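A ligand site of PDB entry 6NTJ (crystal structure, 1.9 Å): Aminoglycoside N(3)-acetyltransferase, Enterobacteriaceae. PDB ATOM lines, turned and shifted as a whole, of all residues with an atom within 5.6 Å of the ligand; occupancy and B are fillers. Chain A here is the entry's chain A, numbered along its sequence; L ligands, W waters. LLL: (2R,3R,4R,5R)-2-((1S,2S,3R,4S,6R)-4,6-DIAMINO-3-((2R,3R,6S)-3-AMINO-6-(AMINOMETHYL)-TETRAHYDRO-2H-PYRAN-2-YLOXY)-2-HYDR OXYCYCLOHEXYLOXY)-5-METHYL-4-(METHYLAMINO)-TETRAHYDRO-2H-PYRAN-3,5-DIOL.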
ATOM      1  N   PHE A  80      -0.225 -11.709  21.240  1.00  0.00           N
ATOM      2  CA  PHE A  80       0.440 -11.805  19.916  1.00  0.00           C
ATOM      3  C   PHE A  80       0.162 -13.220  19.369  1.00  0.00           C
ATOM      4  O   PHE A  80       0.703 -14.238  19.865  1.00  0.00           O
ATOM      5  CB  PHE A  80       1.912 -11.519  20.072  1.00  0.00           C
ATOM      6  CG  PHE A  80       2.749 -11.813  18.844  1.00  0.00           C
ATOM      7  CD1 PHE A  80       3.912 -12.589  18.980  1.00  0.00           C
ATOM      8  CD2 PHE A  80       2.395 -11.348  17.611  1.00  0.00           C
ATOM      9  CE1 PHE A  80       4.720 -12.812  17.884  1.00  0.00           C
ATOM     10  CE2 PHE A  80       3.236 -11.597  16.486  1.00  0.00           C
ATOM     11  CZ  PHE A  80       4.344 -12.349  16.645  1.00  0.00           C
ATOM     12  N   SER A  82      -0.361 -13.922  15.649  1.00  0.00           N
ATOM     13  CA  SER A  82       0.203 -14.159  14.290  1.00  0.00           C
ATOM     14  C   SER A  82      -0.794 -15.044  13.506  1.00  0.00           C
ATOM     15  O   SER A  82      -2.004 -15.050  13.774  1.00  0.00           O
ATOM     16  CB  SER A  82       1.628 -14.711  14.450  1.00  0.00           C
ATOM     17  OG  SER A  82       2.223 -14.809  13.161  1.00  0.00           O
ATOM     18  N   TRP A  83      -0.268 -15.924  12.645  1.00  0.00           N
ATOM     19  CA  TRP A  83      -1.105 -16.617  11.671  1.00  0.00           C
ATOM     20  C   TRP A  83      -0.373 -17.877  11.293  1.00  0.00           C
ATOM     21  O   TRP A  83       0.793 -17.774  10.915  1.00  0.00           O
ATOM     22  CB  TRP A  83      -1.306 -15.758  10.509  1.00  0.00           C
ATOM     23  CG  TRP A  83      -2.097 -16.473   9.319  1.00  0.00           C
ATOM     24  CD1 TRP A  83      -2.938 -17.567   9.401  1.00  0.00           C
ATOM     25  CD2 TRP A  83      -2.046 -16.081   7.950  1.00  0.00           C
ATOM     26  NE1 TRP A  83      -3.420 -17.878   8.102  1.00  0.00           N
ATOM     27  CE2 TRP A  83      -2.908 -16.973   7.219  1.00  0.00           C
ATOM     28  CE3 TRP A  83      -1.398 -15.066   7.261  1.00  0.00           C
ATOM     29  CZ2 TRP A  83      -3.079 -16.839   5.854  1.00  0.00           C
ATOM     30  CZ3 TRP A  83      -1.576 -14.945   5.941  1.00  0.00           C
ATOM     31  CH2 TRP A  83      -2.409 -15.818   5.231  1.00  0.00           C
ATOM     32  N   SER A  86       1.152 -17.811   7.738  1.00  0.00           N
ATOM     33  CA  SER A  86       1.791 -16.619   7.227  1.00  0.00           C
ATOM     34  C   SER A  86       2.847 -17.060   6.194  1.00  0.00           C
ATOM     35  O   SER A  86       3.728 -17.845   6.545  1.00  0.00           O
ATOM     36  CB  SER A  86       2.486 -15.837   8.359  1.00  0.00           C
ATOM     37  OG  SER A  86       3.155 -14.721   7.779  1.00  0.00           O
ATOM     38  N   TYR A  88       5.636 -15.906   5.394  1.00  0.00           N
ATOM     39  CA  TYR A  88       6.730 -14.998   5.670  1.00  0.00           C
ATOM     40  C   TYR A  88       7.997 -15.499   5.027  1.00  0.00           C
ATOM     41  O   TYR A  88       8.639 -14.790   4.239  1.00  0.00           O
ATOM     42  CB  TYR A  88       6.897 -14.869   7.159  1.00  0.00           C
ATOM     43  CG  TYR A  88       8.006 -13.968   7.623  1.00  0.00           C
ATOM     44  CD1 TYR A  88       7.754 -12.604   7.855  1.00  0.00           C
ATOM     45  CD2 TYR A  88       9.280 -14.463   7.841  1.00  0.00           C
ATOM     46  CE1 TYR A  88       8.752 -11.772   8.268  1.00  0.00           C
ATOM     47  CE2 TYR A  88      10.321 -13.626   8.297  1.00  0.00           C
ATOM     48  CZ  TYR A  88      10.026 -12.262   8.499  1.00  0.00           C
ATOM     49  OH  TYR A  88      10.981 -11.329   8.939  1.00  0.00           O
ATOM     50  N   GLU A  89       8.366 -16.755   5.307  1.00  0.00           N
ATOM     51  CA  GLU A  89       9.565 -17.337   4.694  1.00  0.00           C
ATOM     52  C   GLU A  89       9.451 -17.402   3.182  1.00  0.00           C
ATOM     53  O   GLU A  89      10.454 -17.273   2.466  1.00  0.00           O
ATOM     54  CB  GLU A  89       9.796 -18.774   5.213  1.00  0.00           C
ATOM     55  CG  GLU A  89      10.176 -18.963   6.656  1.00  0.00           C
ATOM     56  CD  GLU A  89       9.004 -18.905   7.698  1.00  0.00           C
ATOM     57  OE1 GLU A  89       9.428 -18.929   8.874  1.00  0.00           O
ATOM     58  OE2 GLU A  89       7.740 -18.800   7.364  1.00  0.00           O
ATOM     59  N   TYR A 116      -0.602 -18.763  14.976  1.00  0.00           N
ATOM     60  CA  TYR A 116       0.700 -19.440  14.810  1.00  0.00           C
ATOM     61  C   TYR A 116       1.045 -20.279  16.036  1.00  0.00           C
ATOM     62  O   TYR A 116       1.278 -19.735  17.110  1.00  0.00           O
ATOM     63  CB  TYR A 116       1.783 -18.425  14.530  1.00  0.00           C
ATOM     64  CG  TYR A 116       3.068 -19.113  14.137  1.00  0.00           C
ATOM     65  CD1 TYR A 116       3.207 -19.697  12.874  1.00  0.00           C
ATOM     66  CD2 TYR A 116       4.122 -19.238  15.043  1.00  0.00           C
ATOM     67  CE1 TYR A 116       4.362 -20.325  12.499  1.00  0.00           C
ATOM     68  CE2 TYR A 116       5.325 -19.897  14.656  1.00  0.00           C
ATOM     69  CZ  TYR A 116       5.388 -20.436  13.384  1.00  0.00           C
ATOM     70  OH  TYR A 116       6.548 -21.101  13.001  1.00  0.00           O
ATOM     71  N   GLY A 118       3.651 -21.868  17.187  1.00  0.00           N
ATOM     72  CA  GLY A 118       4.937 -21.662  17.833  1.00  0.00           C
ATOM     73  C   GLY A 118       5.016 -20.527  18.863  1.00  0.00           C
ATOM     74  O   GLY A 118       5.973 -20.488  19.631  1.00  0.00           O
ATOM     75  N   PHE A 119       4.062 -19.589  18.850  1.00  0.00           N
ATOM     76  CA  PHE A 119       4.030 -18.534  19.880  1.00  0.00           C
ATOM     77  C   PHE A 119       3.158 -18.890  21.092  1.00  0.00           C
ATOM     78  O   PHE A 119       2.985 -18.030  21.981  1.00  0.00           O
ATOM     79  CB  PHE A 119       3.556 -17.232  19.266  1.00  0.00           C
ATOM     80  CG  PHE A 119       4.397 -16.802  18.093  1.00  0.00           C
ATOM     81  CD1 PHE A 119       5.759 -17.102  18.046  1.00  0.00           C
ATOM     82  CD2 PHE A 119       3.832 -16.093  17.039  1.00  0.00           C
ATOM     83  CE1 PHE A 119       6.535 -16.700  16.925  1.00  0.00           C
ATOM     84  CE2 PHE A 119       4.630 -15.688  15.954  1.00  0.00           C
ATOM     85  CZ  PHE A 119       5.964 -15.989  15.924  1.00  0.00           C
ATOM     86  N   ASP A 139       0.975 -11.197   9.628  1.00  0.00           N
ATOM     87  CA  ASP A 139       2.083 -11.893  10.264  1.00  0.00           C
ATOM     88  C   ASP A 139       2.256 -11.455  11.711  1.00  0.00           C
ATOM     89  O   ASP A 139       2.678 -12.267  12.561  1.00  0.00           O
ATOM     90  CB  ASP A 139       3.398 -11.638   9.506  1.00  0.00           C
ATOM     91  CG  ASP A 139       4.475 -12.482   9.999  1.00  0.00           C
ATOM     92  OD1 ASP A 139       4.435 -13.760   9.848  1.00  0.00           O
ATOM     93  OD2 ASP A 139       5.396 -11.865  10.562  1.00  0.00           O
ATOM     94  N   TYR A 162       5.451  -3.881  15.011  1.00  0.00           N
ATOM     95  CA  TYR A 162       5.623  -3.781  16.459  1.00  0.00           C
ATOM     96  C   TYR A 162       6.013  -2.381  16.962  1.00  0.00           C
ATOM     97  O   TYR A 162       6.232  -2.184  18.165  1.00  0.00           O
ATOM     98  CB  TYR A 162       6.719  -4.765  16.936  1.00  0.00           C
ATOM     99  CG  TYR A 162       6.474  -6.112  16.374  1.00  0.00           C
ATOM    100  CD1 TYR A 162       7.306  -6.629  15.359  1.00  0.00           C
ATOM    101  CD2 TYR A 162       5.449  -6.912  16.851  1.00  0.00           C
ATOM    102  CE1 TYR A 162       7.076  -7.854  14.829  1.00  0.00           C
ATOM    103  CE2 TYR A 162       5.210  -8.165  16.356  1.00  0.00           C
ATOM    104  CZ  TYR A 162       5.995  -8.632  15.298  1.00  0.00           C
ATOM    105  OH  TYR A 162       5.707  -9.874  14.746  1.00  0.00           O
ATOM    106  N   ASP A 186      13.215 -14.679  25.924  1.00  0.00           N
ATOM    107  CA  ASP A 186      13.054 -14.387  24.521  1.00  0.00           C
ATOM    108  C   ASP A 186      11.623 -14.112  24.080  1.00  0.00           C
ATOM    109  O   ASP A 186      11.392 -13.717  22.904  1.00  0.00           O
ATOM    110  CB  ASP A 186      13.605 -15.554  23.707  1.00  0.00           C
ATOM    111  CG  ASP A 186      12.935 -16.878  24.037  1.00  0.00           C
ATOM    112  OD1 ASP A 186      12.718 -17.175  25.201  1.00  0.00           O
ATOM    113  OD2 ASP A 186      12.593 -17.586  23.100  1.00  0.00           O
ATOM    114  N   HIS A 192      10.261  -5.632  20.758  1.00  0.00           N
ATOM    115  CA  HIS A 192      10.483  -5.221  19.359  1.00  0.00           C
ATOM    116  C   HIS A 192      10.120  -3.763  19.091  1.00  0.00           C
ATOM    117  O   HIS A 192      10.654  -3.187  18.134  1.00  0.00           O
ATOM    118  CB  HIS A 192       9.701  -6.162  18.400  1.00  0.00           C
ATOM    119  CG  HIS A 192      10.265  -7.547  18.413  1.00  0.00           C
ATOM    120  ND1 HIS A 192      11.561  -7.857  18.010  1.00  0.00           N
ATOM    121  CD2 HIS A 192       9.706  -8.705  18.837  1.00  0.00           C
ATOM    122  CE1 HIS A 192      11.770  -9.157  18.192  1.00  0.00           C
ATOM    123  NE2 HIS A 192      10.649  -9.676  18.673  1.00  0.00           N
ATOM    124  N   SER A 228      12.409  -8.545  12.716  1.00  0.00           N
ATOM    125  CA  SER A 228      12.006  -9.019  14.048  1.00  0.00           C
ATOM    126  C   SER A 228      12.758 -10.266  14.450  1.00  0.00           C
ATOM    127  O   SER A 228      12.504 -10.821  15.519  1.00  0.00           O
ATOM    128  CB  SER A 228      10.500  -9.312  14.120  1.00  0.00           C
ATOM    129  OG  SER A 228      10.165 -10.357  13.236  1.00  0.00           O
ATOM    130  N   ASN A 229      13.699 -10.756  13.613  1.00  0.00           N
ATOM    131  CA  ASN A 229      14.520 -11.928  13.972  1.00  0.00           C
ATOM    132  C   ASN A 229      15.992 -11.532  14.181  1.00  0.00           C
ATOM    133  O   ASN A 229      16.910 -12.347  14.019  1.00  0.00           O
ATOM    134  CB  ASN A 229      14.397 -12.974  12.866  1.00  0.00           C
ATOM    135  CG  ASN A 229      13.165 -13.868  13.052  1.00  0.00           C
ATOM    136  OD1 ASN A 229      12.912 -14.396  14.156  1.00  0.00           O
ATOM    137  ND2 ASN A 229      12.404 -14.023  11.995  1.00  0.00           N
ATOM    138  N   GLY A 230      16.223 -10.260  14.444  1.00  0.00           N
ATOM    139  CA  GLY A 230      17.525  -9.781  14.893  1.00  0.00           C
ATOM    140  C   GLY A 230      17.716  -8.384  14.315  1.00  0.00           C
ATOM    141  O   GLY A 230      17.803  -8.232  13.103  1.00  0.00           O
ATOM    142  N   TYR A 235      22.690  -9.967  16.579  1.00  0.00           N
ATOM    143  CA  TYR A 235      21.521 -10.489  17.271  1.00  0.00           C
ATOM    144  C   TYR A 235      20.753 -11.450  16.397  1.00  0.00           C
ATOM    145  O   TYR A 235      19.741 -12.035  16.842  1.00  0.00           O
ATOM    146  CB  TYR A 235      20.613  -9.328  17.699  1.00  0.00           C
ATOM    147  CG  TYR A 235      21.342  -8.437  18.659  1.00  0.00           C
ATOM    148  CD1 TYR A 235      21.504  -7.081  18.409  1.00  0.00           C
ATOM    149  CD2 TYR A 235      21.948  -8.949  19.795  1.00  0.00           C
ATOM    150  CE1 TYR A 235      22.172  -6.253  19.291  1.00  0.00           C
ATOM    151  CE2 TYR A 235      22.658  -8.121  20.660  1.00  0.00           C
ATOM    152  CZ  TYR A 235      22.763  -6.773  20.431  1.00  0.00           C
ATOM    153  OH  TYR A 235      23.443  -5.983  21.329  1.00  0.00           O
ATOM    154  N   ALA A 237      21.866 -14.259  14.682  1.00  0.00           N
ATOM    155  CA  ALA A 237      22.136 -15.696  14.659  1.00  0.00           C
ATOM    156  C   ALA A 237      20.901 -16.459  15.143  1.00  0.00           C
ATOM    157  O   ALA A 237      20.213 -16.003  16.064  1.00  0.00           O
ATOM    158  CB  ALA A 237      23.324 -16.047  15.544  1.00  0.00           C
ATOM    159  N   GLY A 240      22.284 -18.468  19.607  1.00  0.00           N
ATOM    160  CA  GLY A 240      21.828 -17.223  19.041  1.00  0.00           C
ATOM    161  C   GLY A 240      20.814 -16.441  19.885  1.00  0.00           C
ATOM    162  O   GLY A 240      19.635 -16.432  19.444  1.00  0.00           O
ATOM    163  N   ASP A 242      18.880 -13.177  20.728  1.00  0.00           N
ATOM    164  CA  ASP A 242      18.634 -11.945  20.036  1.00  0.00           C
ATOM    165  C   ASP A 242      18.663 -10.815  21.047  1.00  0.00           C
ATOM    166  O   ASP A 242      19.001 -10.982  22.235  1.00  0.00           O
ATOM    167  CB  ASP A 242      17.307 -12.014  19.248  1.00  0.00           C
ATOM    168  CG  ASP A 242      16.078 -12.154  20.131  1.00  0.00           C
ATOM    169  OD1 ASP A 242      16.162 -12.408  21.358  1.00  0.00           O
ATOM    170  OD2 ASP A 242      14.979 -12.002  19.577  1.00  0.00           O
ATOM    171  N   VAL A 244      16.122  -9.104  22.079  1.00  0.00           N
ATOM    172  CA  VAL A 244      15.025  -9.189  23.057  1.00  0.00           C
ATOM    173  C   VAL A 244      15.502  -9.948  24.259  1.00  0.00           C
ATOM    174  O   VAL A 244      15.346  -9.511  25.409  1.00  0.00           O
ATOM    175  CB  VAL A 244      13.759  -9.874  22.442  1.00  0.00           C
ATOM    176  CG1 VAL A 244      12.710 -10.107  23.560  1.00  0.00           C
ATOM    177  CG2 VAL A 244      13.270  -8.968  21.323  1.00  0.00           C
HETATM  178  C11 LLL L   1      11.781 -16.507  17.616  1.00  0.00           C
HETATM  179  O11 LLL L   1      11.019 -15.264  17.926  1.00  0.00           O
HETATM  180  C21 LLL L   1      11.721 -17.376  18.893  1.00  0.00           C
HETATM  181  N21 LLL L   1      10.303 -17.544  19.286  1.00  0.00           N
HETATM  182  C31 LLL L   1      12.400 -16.620  20.037  1.00  0.00           C
HETATM  183  C41 LLL L   1      13.859 -16.350  19.607  1.00  0.00           C
HETATM  184  C51 LLL L   1      13.811 -15.525  18.315  1.00  0.00           C
HETATM  185  O51 LLL L   1      13.136 -16.220  17.236  1.00  0.00           O
HETATM  186  C61 LLL L   1      15.265 -15.340  17.890  1.00  0.00           C
HETATM  187  N61 LLL L   1      15.197 -14.929  16.524  1.00  0.00           N
HETATM  188  C12 LLL L   1       8.662 -12.857  15.583  1.00  0.00           C
HETATM  189  N12 LLL L   1       7.997 -11.967  14.654  1.00  0.00           N
HETATM  190  C22 LLL L   1       9.554 -12.083  16.573  1.00  0.00           C
HETATM  191  C32 LLL L   1      10.031 -13.160  17.552  1.00  0.00           C
HETATM  192  N32 LLL L   1      10.891 -12.555  18.624  1.00  0.00           N
HETATM  193  C42 LLL L   1      10.853 -14.302  16.856  1.00  0.00           C
HETATM  194  C52 LLL L   1      10.051 -14.877  15.707  1.00  0.00           C
HETATM  195  O52 LLL L   1      10.904 -15.753  14.925  1.00  0.00           O
HETATM  196  C62 LLL L   1       9.480 -13.832  14.769  1.00  0.00           C
HETATM  197  O62 LLL L   1       8.658 -14.510  13.758  1.00  0.00           O
HETATM  198  C13 LLL L   1       8.862 -14.163  12.433  1.00  0.00           C
HETATM  199  C23 LLL L   1       7.525 -14.383  11.696  1.00  0.00           C
HETATM  200  O23 LLL L   1       6.563 -13.424  12.229  1.00  0.00           O
HETATM  201  C33 LLL L   1       6.958 -15.851  11.762  1.00  0.00           C
HETATM  202  N33 LLL L   1       5.765 -15.910  10.864  1.00  0.00           N
HETATM  203  C43 LLL L   1       8.091 -16.815  11.317  1.00  0.00           C
HETATM  204  O43 LLL L   1       8.115 -16.731   9.890  1.00  0.00           O
HETATM  205  C53 LLL L   1       9.454 -16.396  11.936  1.00  0.00           C
HETATM  206  O53 LLL L   1       9.830 -15.024  11.749  1.00  0.00           O
HETATM  207  C83 LLL L   1       7.712 -18.249  11.686  1.00  0.00           C
HETATM  208  C93 LLL L   1       4.611 -16.528  11.590  1.00  0.00           C
HETATM  209  O   HOH W   1       9.604 -15.018  21.086  1.00  0.00           O
HETATM  210  O   HOH W   2       5.331 -18.069   8.949  1.00  0.00           O
HETATM  211  O   HOH W   3       9.734 -12.113  21.420  1.00  0.00           O
HETATM  212  O   HOH W   4      18.361 -14.202  16.499  1.00  0.00           O
HETATM  213  O   HOH W   5      13.758 -12.235  17.282  1.00  0.00           O
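OG of Ser 82 touches C93 of the ligand, at 3.3 Å.
CB of Ser 86 touches C93 of the ligand (3.9 Å).
CD2 of Tyr 88 touches O43 of the ligand, at 3.3 Å.
Tyr 116 touches the ligand (OH to C83, 3.3 Å).
Phe 119 touches the ligand (CZ to O62, 3.8 Å).
OD2 of Asp 186 touches C31 of the ligand, at 3.2 Å.
Asp 242 touches the ligand (OD2 to C61, 3.8 Å).
13 residues have an atom within 4 Å of the ligand: Ser 82, Ser 86, Tyr 88, Glu 89, Tyr 116, Phe 119, Asp 139, Tyr 162, Asp 186, His 192, Ser 228, Asn 229 and Asp 242.
The nearest printed residue that does not touch the ligand is Trp 83 (4.1 Å).
The side-chain hydroxyl (OG) of Ser 86 is in hydrogen-bond range of the side-chain carboxylate (OD1) of Asp 139 (2.6 Å).
The backbone NH of Val 244 sits close to the side-chain carboxylate of Asp 242, 3.4 Å away.
The side-chain hydroxyl (OG) of Ser 82 sits at hydrogen-bond distance from the backbone carbonyl oxygen (O) of Asp 139.
The side-chain hydroxyl of Ser 228 lies within hydrogen-bond range of a nitrogen (N12) of the ligand, 3.1 Å away.
The side-chain amide oxygen (OD1) of Asn 229 lies within hydrogen-bond range of an oxygen (O52) of the ligand (2.5 Å).
The side-chain carboxylate (OE1) of Glu 89 sits at hydrogen-bond distance from an oxygen (O43) of the ligand (2.8 Å).
N32 of the ligand sits at hydrogen-bond distance from NE2 of His 192, at 2.9 Å.
OH of Tyr 162 is in hydrogen-bond range of N12 of the ligand.
The side-chain carboxylate of Asp 139 lies within salt-bridge range of a nitrogen (N33) of the ligand (2.7 Å).
Water W2 lies within hydrogen-bond range of O of Ser 86, N33 of the ligand and OE2 of Glu 89.
Water W3 lies within hydrogen-bond range of O of Asp 186 and N32 of the ligand.
Water W5 lies within hydrogen-bond range of O of Ser 228 (2.6 Å), OD2 of Asp 242 (2.6 Å) and N61 of the ligand (3.1 Å).
Water W1 bridges O of Asp 186 (2.9 Å) and N21 of the ligand (3.2 Å).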
